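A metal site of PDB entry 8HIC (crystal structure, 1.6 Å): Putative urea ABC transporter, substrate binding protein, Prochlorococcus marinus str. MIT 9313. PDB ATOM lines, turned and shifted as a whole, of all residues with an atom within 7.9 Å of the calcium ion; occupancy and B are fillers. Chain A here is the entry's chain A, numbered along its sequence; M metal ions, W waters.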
ATOM      1  N   TYR A 118      17.535 -29.784 -18.708  1.00  0.00           N
ATOM      2  CA  TYR A 118      17.950 -31.010 -19.406  1.00  0.00           C
ATOM      3  C   TYR A 118      18.281 -30.669 -20.849  1.00  0.00           C
ATOM      4  O   TYR A 118      17.425 -30.122 -21.563  1.00  0.00           O
ATOM      5  CB  TYR A 118      16.812 -32.041 -19.329  1.00  0.00           C
ATOM      6  CG  TYR A 118      16.942 -33.244 -20.234  1.00  0.00           C
ATOM      7  CD1 TYR A 118      17.830 -34.260 -19.940  1.00  0.00           C
ATOM      8  CD2 TYR A 118      16.127 -33.391 -21.355  1.00  0.00           C
ATOM      9  CE1 TYR A 118      17.936 -35.382 -20.757  1.00  0.00           C
ATOM     10  CE2 TYR A 118      16.226 -34.497 -22.177  1.00  0.00           C
ATOM     11  CZ  TYR A 118      17.121 -35.491 -21.862  1.00  0.00           C
ATOM     12  OH  TYR A 118      17.220 -36.601 -22.675  1.00  0.00           O
ATOM     13  N   PRO A 119      19.481 -30.978 -21.339  1.00  0.00           N
ATOM     14  CA  PRO A 119      19.919 -30.465 -22.656  1.00  0.00           C
ATOM     15  C   PRO A 119      19.797 -31.411 -23.852  1.00  0.00           C
ATOM     16  O   PRO A 119      20.092 -30.962 -24.957  1.00  0.00           O
ATOM     17  CB  PRO A 119      21.406 -30.159 -22.387  1.00  0.00           C
ATOM     18  CG  PRO A 119      21.827 -31.244 -21.427  1.00  0.00           C
ATOM     19  CD  PRO A 119      20.614 -31.483 -20.531  1.00  0.00           C
ATOM     20  N   ILE A 120      19.380 -32.663 -23.706  1.00  0.00           N
ATOM     21  CA  ILE A 120      19.631 -33.638 -24.766  1.00  0.00           C
ATOM     22  C   ILE A 120      18.388 -33.905 -25.612  1.00  0.00           C
ATOM     23  O   ILE A 120      17.262 -33.957 -25.109  1.00  0.00           O
ATOM     24  CB  ILE A 120      20.212 -34.937 -24.171  1.00  0.00           C
ATOM     25  CG1 ILE A 120      21.544 -34.629 -23.475  1.00  0.00           C
ATOM     26  CG2 ILE A 120      20.378 -35.988 -25.258  1.00  0.00           C
ATOM     27  CD1 ILE A 120      22.496 -33.786 -24.315  1.00  0.00           C
ATOM     28  N   GLN A 121      18.611 -34.030 -26.938  1.00  0.00           N
ATOM     29  CA  GLN A 121      17.592 -34.478 -27.889  1.00  0.00           C
ATOM     30  C   GLN A 121      16.840 -35.662 -27.313  1.00  0.00           C
ATOM     31  O   GLN A 121      17.454 -36.561 -26.716  1.00  0.00           O
ATOM     32  CB  GLN A 121      18.229 -34.940 -29.209  1.00  0.00           C
ATOM     33  CG  GLN A 121      19.467 -35.843 -29.025  1.00  0.00           C
ATOM     34  CD  GLN A 121      19.146 -37.337 -28.889  1.00  0.00           C
ATOM     35  OE1 GLN A 121      18.147 -37.824 -29.418  1.00  0.00           O
ATOM     36  NE2 GLN A 121      19.962 -38.033 -28.123  1.00  0.00           N
ATOM     37  N   TYR A 133      13.929 -27.751 -21.175  1.00  0.00           N
ATOM     38  CA  TYR A 133      14.520 -28.598 -22.197  1.00  0.00           C
ATOM     39  C   TYR A 133      15.161 -27.750 -23.287  1.00  0.00           C
ATOM     40  O   TYR A 133      14.491 -26.904 -23.879  1.00  0.00           O
ATOM     41  CB  TYR A 133      13.464 -29.514 -22.850  1.00  0.00           C
ATOM     42  CG  TYR A 133      12.549 -30.278 -21.908  1.00  0.00           C
ATOM     43  CD1 TYR A 133      11.516 -29.639 -21.229  1.00  0.00           C
ATOM     44  CD2 TYR A 133      12.670 -31.655 -21.753  1.00  0.00           C
ATOM     45  CE1 TYR A 133      10.662 -30.356 -20.382  1.00  0.00           C
ATOM     46  CE2 TYR A 133      11.827 -32.367 -20.925  1.00  0.00           C
ATOM     47  CZ  TYR A 133      10.828 -31.719 -20.240  1.00  0.00           C
ATOM     48  OH  TYR A 133       9.978 -32.423 -19.398  1.00  0.00           O
ATOM     49  N   THR A 134      16.439 -28.000 -23.581  1.00  0.00           N
ATOM     50  CA  THR A 134      17.071 -27.386 -24.752  1.00  0.00           C
ATOM     51  C   THR A 134      17.417 -28.386 -25.848  1.00  0.00           C
ATOM     52  O   THR A 134      17.908 -27.986 -26.905  1.00  0.00           O
ATOM     53  CB  THR A 134      18.344 -26.612 -24.362  1.00  0.00           C
ATOM     54  OG1 THR A 134      19.261 -27.485 -23.676  1.00  0.00           O
ATOM     55  CG2 THR A 134      18.024 -25.375 -23.500  1.00  0.00           C
ATOM     56  N   GLY A 135      17.148 -29.677 -25.642  1.00  0.00           N
ATOM     57  CA  GLY A 135      17.363 -30.633 -26.696  1.00  0.00           C
ATOM     58  C   GLY A 135      16.183 -30.699 -27.647  1.00  0.00           C
ATOM     59  O   GLY A 135      15.045 -30.406 -27.290  1.00  0.00           O
ATOM     60  N   ALA A 136      16.475 -31.105 -28.882  1.00  0.00           N
ATOM     61  CA  ALA A 136      15.436 -31.252 -29.900  1.00  0.00           C
ATOM     62  C   ALA A 136      14.327 -32.207 -29.460  1.00  0.00           C
ATOM     63  O   ALA A 136      14.590 -33.267 -28.895  1.00  0.00           O
ATOM     64  CB  ALA A 136      16.059 -31.765 -31.200  1.00  0.00           C
ATOM     65  N   THR A 137      13.084 -31.814 -29.724  1.00  0.00           N
ATOM     66  CA  THR A 137      11.969 -32.742 -29.787  1.00  0.00           C
ATOM     67  C   THR A 137      11.978 -33.418 -31.161  1.00  0.00           C
ATOM     68  O   THR A 137      12.704 -32.993 -32.057  1.00  0.00           O
ATOM     69  CB  THR A 137      10.654 -31.995 -29.553  1.00  0.00           C
ATOM     70  OG1 THR A 137      10.545 -30.914 -30.491  1.00  0.00           O
ATOM     71  CG2 THR A 137      10.620 -31.448 -28.127  1.00  0.00           C
ATOM     72  N   GLN A 140      11.930 -31.433 -34.314  1.00  0.00           N
ATOM     73  CA  GLN A 140      13.156 -30.687 -34.530  1.00  0.00           C
ATOM     74  C   GLN A 140      14.351 -31.582 -34.859  1.00  0.00           C
ATOM     75  O   GLN A 140      15.472 -31.078 -34.947  1.00  0.00           O
ATOM     76  CB  GLN A 140      13.502 -29.840 -33.294  1.00  0.00           C
ATOM     77  CG  GLN A 140      12.392 -28.885 -32.856  1.00  0.00           C
ATOM     78  CD  GLN A 140      12.742 -28.139 -31.576  1.00  0.00           C
ATOM     79  OE1 GLN A 140      13.170 -28.732 -30.598  1.00  0.00           O
ATOM     80  NE2 GLN A 140      12.559 -26.821 -31.586  1.00  0.00           N
ATOM     81  N   TRP A 272      20.450 -32.275 -36.460  1.00  0.00           N
ATOM     82  CA  TRP A 272      20.760 -31.553 -35.227  1.00  0.00           C
ATOM     83  C   TRP A 272      20.361 -30.096 -35.368  1.00  0.00           C
ATOM     84  O   TRP A 272      20.109 -29.593 -36.470  1.00  0.00           O
ATOM     85  CB  TRP A 272      22.257 -31.656 -34.894  1.00  0.00           C
ATOM     86  CG  TRP A 272      22.715 -33.020 -34.522  1.00  0.00           C
ATOM     87  CD1 TRP A 272      23.416 -33.894 -35.285  1.00  0.00           C
ATOM     88  CD2 TRP A 272      22.481 -33.679 -33.274  1.00  0.00           C
ATOM     89  NE1 TRP A 272      23.644 -35.060 -34.593  1.00  0.00           N
ATOM     90  CE2 TRP A 272      23.079 -34.949 -33.353  1.00  0.00           C
ATOM     91  CE3 TRP A 272      21.822 -33.307 -32.093  1.00  0.00           C
ATOM     92  CZ2 TRP A 272      23.057 -35.855 -32.284  1.00  0.00           C
ATOM     93  CZ3 TRP A 272      21.794 -34.193 -31.037  1.00  0.00           C
ATOM     94  CH2 TRP A 272      22.426 -35.455 -31.131  1.00  0.00           C
ATOM     95  N   ASN A 273      20.359 -29.388 -34.242  1.00  0.00           N
ATOM     96  CA  ASN A 273      20.111 -27.964 -34.288  1.00  0.00           C
ATOM     97  C   ASN A 273      21.390 -27.139 -34.312  1.00  0.00           C
ATOM     98  O   ASN A 273      21.418 -26.072 -34.940  1.00  0.00           O
ATOM     99  CB  ASN A 273      19.218 -27.576 -33.106  1.00  0.00           C
ATOM    100  CG  ASN A 273      18.037 -28.509 -32.990  1.00  0.00           C
ATOM    101  OD1 ASN A 273      17.936 -29.272 -32.028  1.00  0.00           O
ATOM    102  ND2 ASN A 273      17.172 -28.487 -33.998  1.00  0.00           N
ATOM    103  N   TYR A 274      22.459 -27.617 -33.694  1.00  0.00           N
ATOM    104  CA  TYR A 274      23.779 -27.032 -33.820  1.00  0.00           C
ATOM    105  C   TYR A 274      24.719 -28.034 -34.466  1.00  0.00           C
ATOM    106  O   TYR A 274      24.669 -29.233 -34.160  1.00  0.00           O
ATOM    107  CB  TYR A 274      24.361 -26.577 -32.463  1.00  0.00           C
ATOM    108  CG  TYR A 274      25.747 -26.005 -32.632  1.00  0.00           C
ATOM    109  CD1 TYR A 274      25.932 -24.735 -33.159  1.00  0.00           C
ATOM    110  CD2 TYR A 274      26.866 -26.765 -32.329  1.00  0.00           C
ATOM    111  CE1 TYR A 274      27.196 -24.222 -33.364  1.00  0.00           C
ATOM    112  CE2 TYR A 274      28.148 -26.262 -32.526  1.00  0.00           C
ATOM    113  CZ  TYR A 274      28.304 -24.984 -33.052  1.00  0.00           C
ATOM    114  OH  TYR A 274      29.555 -24.477 -33.260  1.00  0.00           O
ATOM    115  N   ALA A 301      29.542 -29.423 -30.512  1.00  0.00           N
ATOM    116  CA  ALA A 301      28.478 -30.230 -31.097  1.00  0.00           C
ATOM    117  C   ALA A 301      27.165 -29.834 -30.447  1.00  0.00           C
ATOM    118  O   ALA A 301      27.135 -29.134 -29.435  1.00  0.00           O
ATOM    119  CB  ALA A 301      28.745 -31.721 -30.893  1.00  0.00           C
ATOM    120  N   ASP A 302      26.070 -30.357 -31.010  1.00  0.00           N
ATOM    121  CA  ASP A 302      24.732 -30.022 -30.508  1.00  0.00           C
ATOM    122  C   ASP A 302      24.534 -30.306 -29.030  1.00  0.00           C
ATOM    123  O   ASP A 302      23.963 -29.440 -28.337  1.00  0.00           O
ATOM    124  CB  ASP A 302      23.690 -30.747 -31.362  1.00  0.00           C
ATOM    125  CG  ASP A 302      22.271 -30.341 -31.011  1.00  0.00           C
ATOM    126  OD1 ASP A 302      21.778 -30.783 -29.962  1.00  0.00           O
ATOM    127  OD2 ASP A 302      21.672 -29.582 -31.788  1.00  0.00           O
ATOM    128  N   PRO A 303      24.914 -31.466 -28.476  1.00  0.00           N
ATOM    129  CA  PRO A 303      24.686 -31.665 -27.039  1.00  0.00           C
ATOM    130  C   PRO A 303      25.361 -30.584 -26.212  1.00  0.00           C
ATOM    131  O   PRO A 303      24.765 -30.065 -25.246  1.00  0.00           O
ATOM    132  CB  PRO A 303      25.287 -33.053 -26.787  1.00  0.00           C
ATOM    133  CG  PRO A 303      25.104 -33.759 -28.091  1.00  0.00           C
ATOM    134  CD  PRO A 303      25.425 -32.694 -29.112  1.00  0.00           C
ATOM    135  N   GLN A 304      26.577 -30.207 -26.589  1.00  0.00           N
ATOM    136  CA  GLN A 304      27.292 -29.148 -25.867  1.00  0.00           C
ATOM    137  C   GLN A 304      26.619 -27.806 -26.046  1.00  0.00           C
ATOM    138  O   GLN A 304      26.487 -27.051 -25.084  1.00  0.00           O
ATOM    139  CB  GLN A 304      28.740 -29.067 -26.354  1.00  0.00           C
ATOM    140  CG  GLN A 304      29.591 -30.233 -25.931  1.00  0.00           C
ATOM    141  CD  GLN A 304      30.805 -30.357 -26.809  1.00  0.00           C
ATOM    142  OE1 GLN A 304      30.874 -31.197 -27.693  1.00  0.00           O
ATOM    143  NE2 GLN A 304      31.787 -29.485 -26.585  1.00  0.00           N
ATOM    144  N   GLU A 305      26.219 -27.468 -27.286  1.00  0.00           N
ATOM    145  CA  GLU A 305      25.527 -26.212 -27.537  1.00  0.00           C
ATOM    146  C   GLU A 305      24.245 -26.133 -26.716  1.00  0.00           C
ATOM    147  O   GLU A 305      23.929 -25.089 -26.134  1.00  0.00           O
ATOM    148  CB  GLU A 305      25.237 -26.064 -29.036  1.00  0.00           C
ATOM    149  CG  GLU A 305      24.951 -24.636 -29.465  1.00  0.00           C
ATOM    150  CD  GLU A 305      23.468 -24.309 -29.547  1.00  0.00           C
ATOM    151  OE1 GLU A 305      22.609 -25.216 -29.406  1.00  0.00           O
ATOM    152  OE2 GLU A 305      23.165 -23.121 -29.765  1.00  0.00           O
ATOM    153  N   SER A 306      23.521 -27.249 -26.633  1.00  0.00           N
ATOM    154  CA  SER A 306      22.316 -27.299 -25.830  1.00  0.00           C
ATOM    155  C   SER A 306      22.605 -27.011 -24.360  1.00  0.00           C
ATOM    156  O   SER A 306      21.878 -26.247 -23.713  1.00  0.00           O
ATOM    157  CB  SER A 306      21.653 -28.669 -25.984  1.00  0.00           C
ATOM    158  OG  SER A 306      21.309 -28.912 -27.340  1.00  0.00           O
ATOM    159  N   ALA A 307      23.667 -27.612 -23.818  1.00  0.00           N
ATOM    160  CA  ALA A 307      23.994 -27.439 -22.395  1.00  0.00           C
ATOM    161  C   ALA A 307      24.506 -26.034 -22.118  1.00  0.00           C
ATOM    162  O   ALA A 307      24.165 -25.439 -21.088  1.00  0.00           O
ATOM    163  CB  ALA A 307      25.026 -28.480 -21.970  1.00  0.00           C
ATOM    164  N   ASN A 309      23.627 -23.324 -23.720  1.00  0.00           N
ATOM    165  CA  ASN A 309      22.454 -22.477 -23.726  1.00  0.00           C
ATOM    166  C   ASN A 309      21.694 -22.515 -22.403  1.00  0.00           C
ATOM    167  O   ASN A 309      21.179 -21.491 -21.943  1.00  0.00           O
ATOM    168  CB  ASN A 309      21.544 -22.874 -24.887  1.00  0.00           C
ATOM    169  CG  ASN A 309      22.123 -22.482 -26.235  1.00  0.00           C
ATOM    170  OD1 ASN A 309      23.129 -21.764 -26.315  1.00  0.00           O
ATOM    171  ND2 ASN A 309      21.495 -22.965 -27.301  1.00  0.00           N
ATOM    172  N   GLN A 342      24.077 -21.671 -32.278  1.00  0.00           N
ATOM    173  CA  GLN A 342      23.312 -22.182 -33.412  1.00  0.00           C
ATOM    174  C   GLN A 342      22.534 -21.105 -34.163  1.00  0.00           C
ATOM    175  O   GLN A 342      22.029 -21.373 -35.257  1.00  0.00           O
ATOM    176  CB  GLN A 342      22.318 -23.248 -32.956  1.00  0.00           C
ATOM    177  CG  GLN A 342      21.105 -22.666 -32.207  1.00  0.00           C
ATOM    178  CD  GLN A 342      19.980 -23.668 -32.051  1.00  0.00           C
ATOM    179  OE1 GLN A 342      18.956 -23.564 -32.730  1.00  0.00           O
ATOM    180  NE2 GLN A 342      20.165 -24.652 -31.174  1.00  0.00           N
ATOM    181  N   VAL A 345      17.583 -18.618 -30.295  1.00  0.00           N
ATOM    182  CA  VAL A 345      16.726 -19.605 -29.631  1.00  0.00           C
ATOM    183  C   VAL A 345      15.804 -18.884 -28.657  1.00  0.00           C
ATOM    184  O   VAL A 345      16.084 -17.771 -28.207  1.00  0.00           O
ATOM    185  CB  VAL A 345      17.548 -20.701 -28.918  1.00  0.00           C
ATOM    186  CG1 VAL A 345      18.442 -21.410 -29.922  1.00  0.00           C
ATOM    187  CG2 VAL A 345      18.377 -20.118 -27.759  1.00  0.00           C
ATOM    188  N   LEU A 353      12.581 -25.504 -26.489  1.00  0.00           N
ATOM    189  CA  LEU A 353      13.352 -24.425 -27.098  1.00  0.00           C
ATOM    190  C   LEU A 353      13.079 -24.366 -28.590  1.00  0.00           C
ATOM    191  O   LEU A 353      13.170 -25.378 -29.285  1.00  0.00           O
ATOM    192  CB  LEU A 353      14.852 -24.650 -26.850  1.00  0.00           C
ATOM    193  CG  LEU A 353      15.770 -23.450 -27.100  1.00  0.00           C
ATOM    194  CD1 LEU A 353      15.596 -22.392 -26.021  1.00  0.00           C
ATOM    195  CD2 LEU A 353      17.208 -23.910 -27.146  1.00  0.00           C
ATOM    196  N   SER A 354      12.718 -23.185 -29.100  1.00  0.00           N
ATOM    197  CA  SER A 354      12.620 -23.029 -30.548  1.00  0.00           C
ATOM    198  C   SER A 354      14.020 -22.953 -31.140  1.00  0.00           C
ATOM    199  O   SER A 354      14.902 -22.260 -30.607  1.00  0.00           O
ATOM    200  CB  SER A 354      11.793 -21.788 -30.926  1.00  0.00           C
ATOM    201  OG  SER A 354      12.419 -20.590 -30.521  1.00  0.00           O
ATOM    202  N   GLN A 355      14.246 -23.722 -32.210  1.00  0.00           N
ATOM    203  CA  GLN A 355      15.592 -23.994 -32.705  1.00  0.00           C
ATOM    204  C   GLN A 355      15.555 -24.234 -34.200  1.00  0.00           C
ATOM    205  O   GLN A 355      14.566 -24.754 -34.742  1.00  0.00           O
ATOM    206  CB  GLN A 355      16.217 -25.227 -32.034  1.00  0.00           C
ATOM    207  CG  GLN A 355      16.284 -25.175 -30.520  1.00  0.00           C
ATOM    208  CD  GLN A 355      16.938 -26.402 -29.931  1.00  0.00           C
ATOM    209  OE1 GLN A 355      18.152 -26.500 -29.891  1.00  0.00           O
ATOM    210  NE2 GLN A 355      16.118 -27.339 -29.450  1.00  0.00           N
ATOM    211  N   THR A 356      16.644 -23.888 -34.873  1.00  0.00           N
ATOM    212  CA  THR A 356      16.819 -24.162 -36.290  1.00  0.00           C
ATOM    213  C   THR A 356      17.224 -25.615 -36.485  1.00  0.00           C
ATOM    214  O   THR A 356      17.936 -26.175 -35.646  1.00  0.00           O
ATOM    215  CB  THR A 356      17.897 -23.223 -36.849  1.00  0.00           C
ATOM    216  OG1 THR A 356      17.472 -21.872 -36.666  1.00  0.00           O
ATOM    217  CG2 THR A 356      18.156 -23.487 -38.320  1.00  0.00           C
HETATM  218 CA    CA M   1      19.545 -27.890 -28.551  1.00  0.00          CA
HETATM  219  O   HOH W   1      19.089 -29.993 -29.739  1.00  0.00           O
HETATM  220  O   HOH W   2      21.220 -27.415 -30.150  1.00  0.00           O
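N of Tyr 274 sits at hydrogen-bond distance from OD2 of Asp 302 (2.8 Å).
NE2 of Gln 355 sits at hydrogen-bond distance from OE1 of Gln 140, at 3.5 Å.
O of Tyr 118 lies within hydrogen-bond range of N of Thr 134, 3.1 Å away.
The backbone carbonyl oxygen (O) of Asp 302 sits close to the side-chain hydroxyl (OG) of Ser 306, 2.9 Å away.
The side-chain carboxylate (OD2) of Asp 302 lies within hydrogen-bond range of the backbone NH (N) of Asn 273, at 2.8 Å.
The backbone NH of Gly 135 sits close to the backbone carbonyl oxygen of Pro 119 (3.3 Å).
The backbone carbonyl oxygen (O) of Pro 119 lies close to the side-chain hydroxyl (OG) of Ser 306, at 3.4 Å.
The side-chain amide oxygen of Gln 355 sits close to the side-chain amide nitrogen of Gln 342.
Gly 135 touches the calcium ion (CA to CA, 3.97 Å).
Asp 302 touches the calcium ion (OD1 to CA, 3.9 Å).
The calcium ion is bound by O of Thr 134 (2.3 Å), water W2 (2.4 Å), OG of Ser 306 (2.4 Å), OE1 of Gln 355 (2.4 Å) and water W1 (2.5 Å).
Water W2 lies within hydrogen-bond range of the side-chain carboxylate of Glu 305 (2.7 Å), the side-chain carboxylate of Asp 302 (2.8 Å) and the side-chain amide nitrogen of Gln 342 (3.1 Å).
Water W1 lies within hydrogen-bond range of the side-chain amide oxygen (OD1) of Asn 273 (2.7 Å), the side-chain carboxylate (OD1) of Asp 302 (2.8 Å) and the backbone NH (N) of Ala 136 (3.0 Å).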
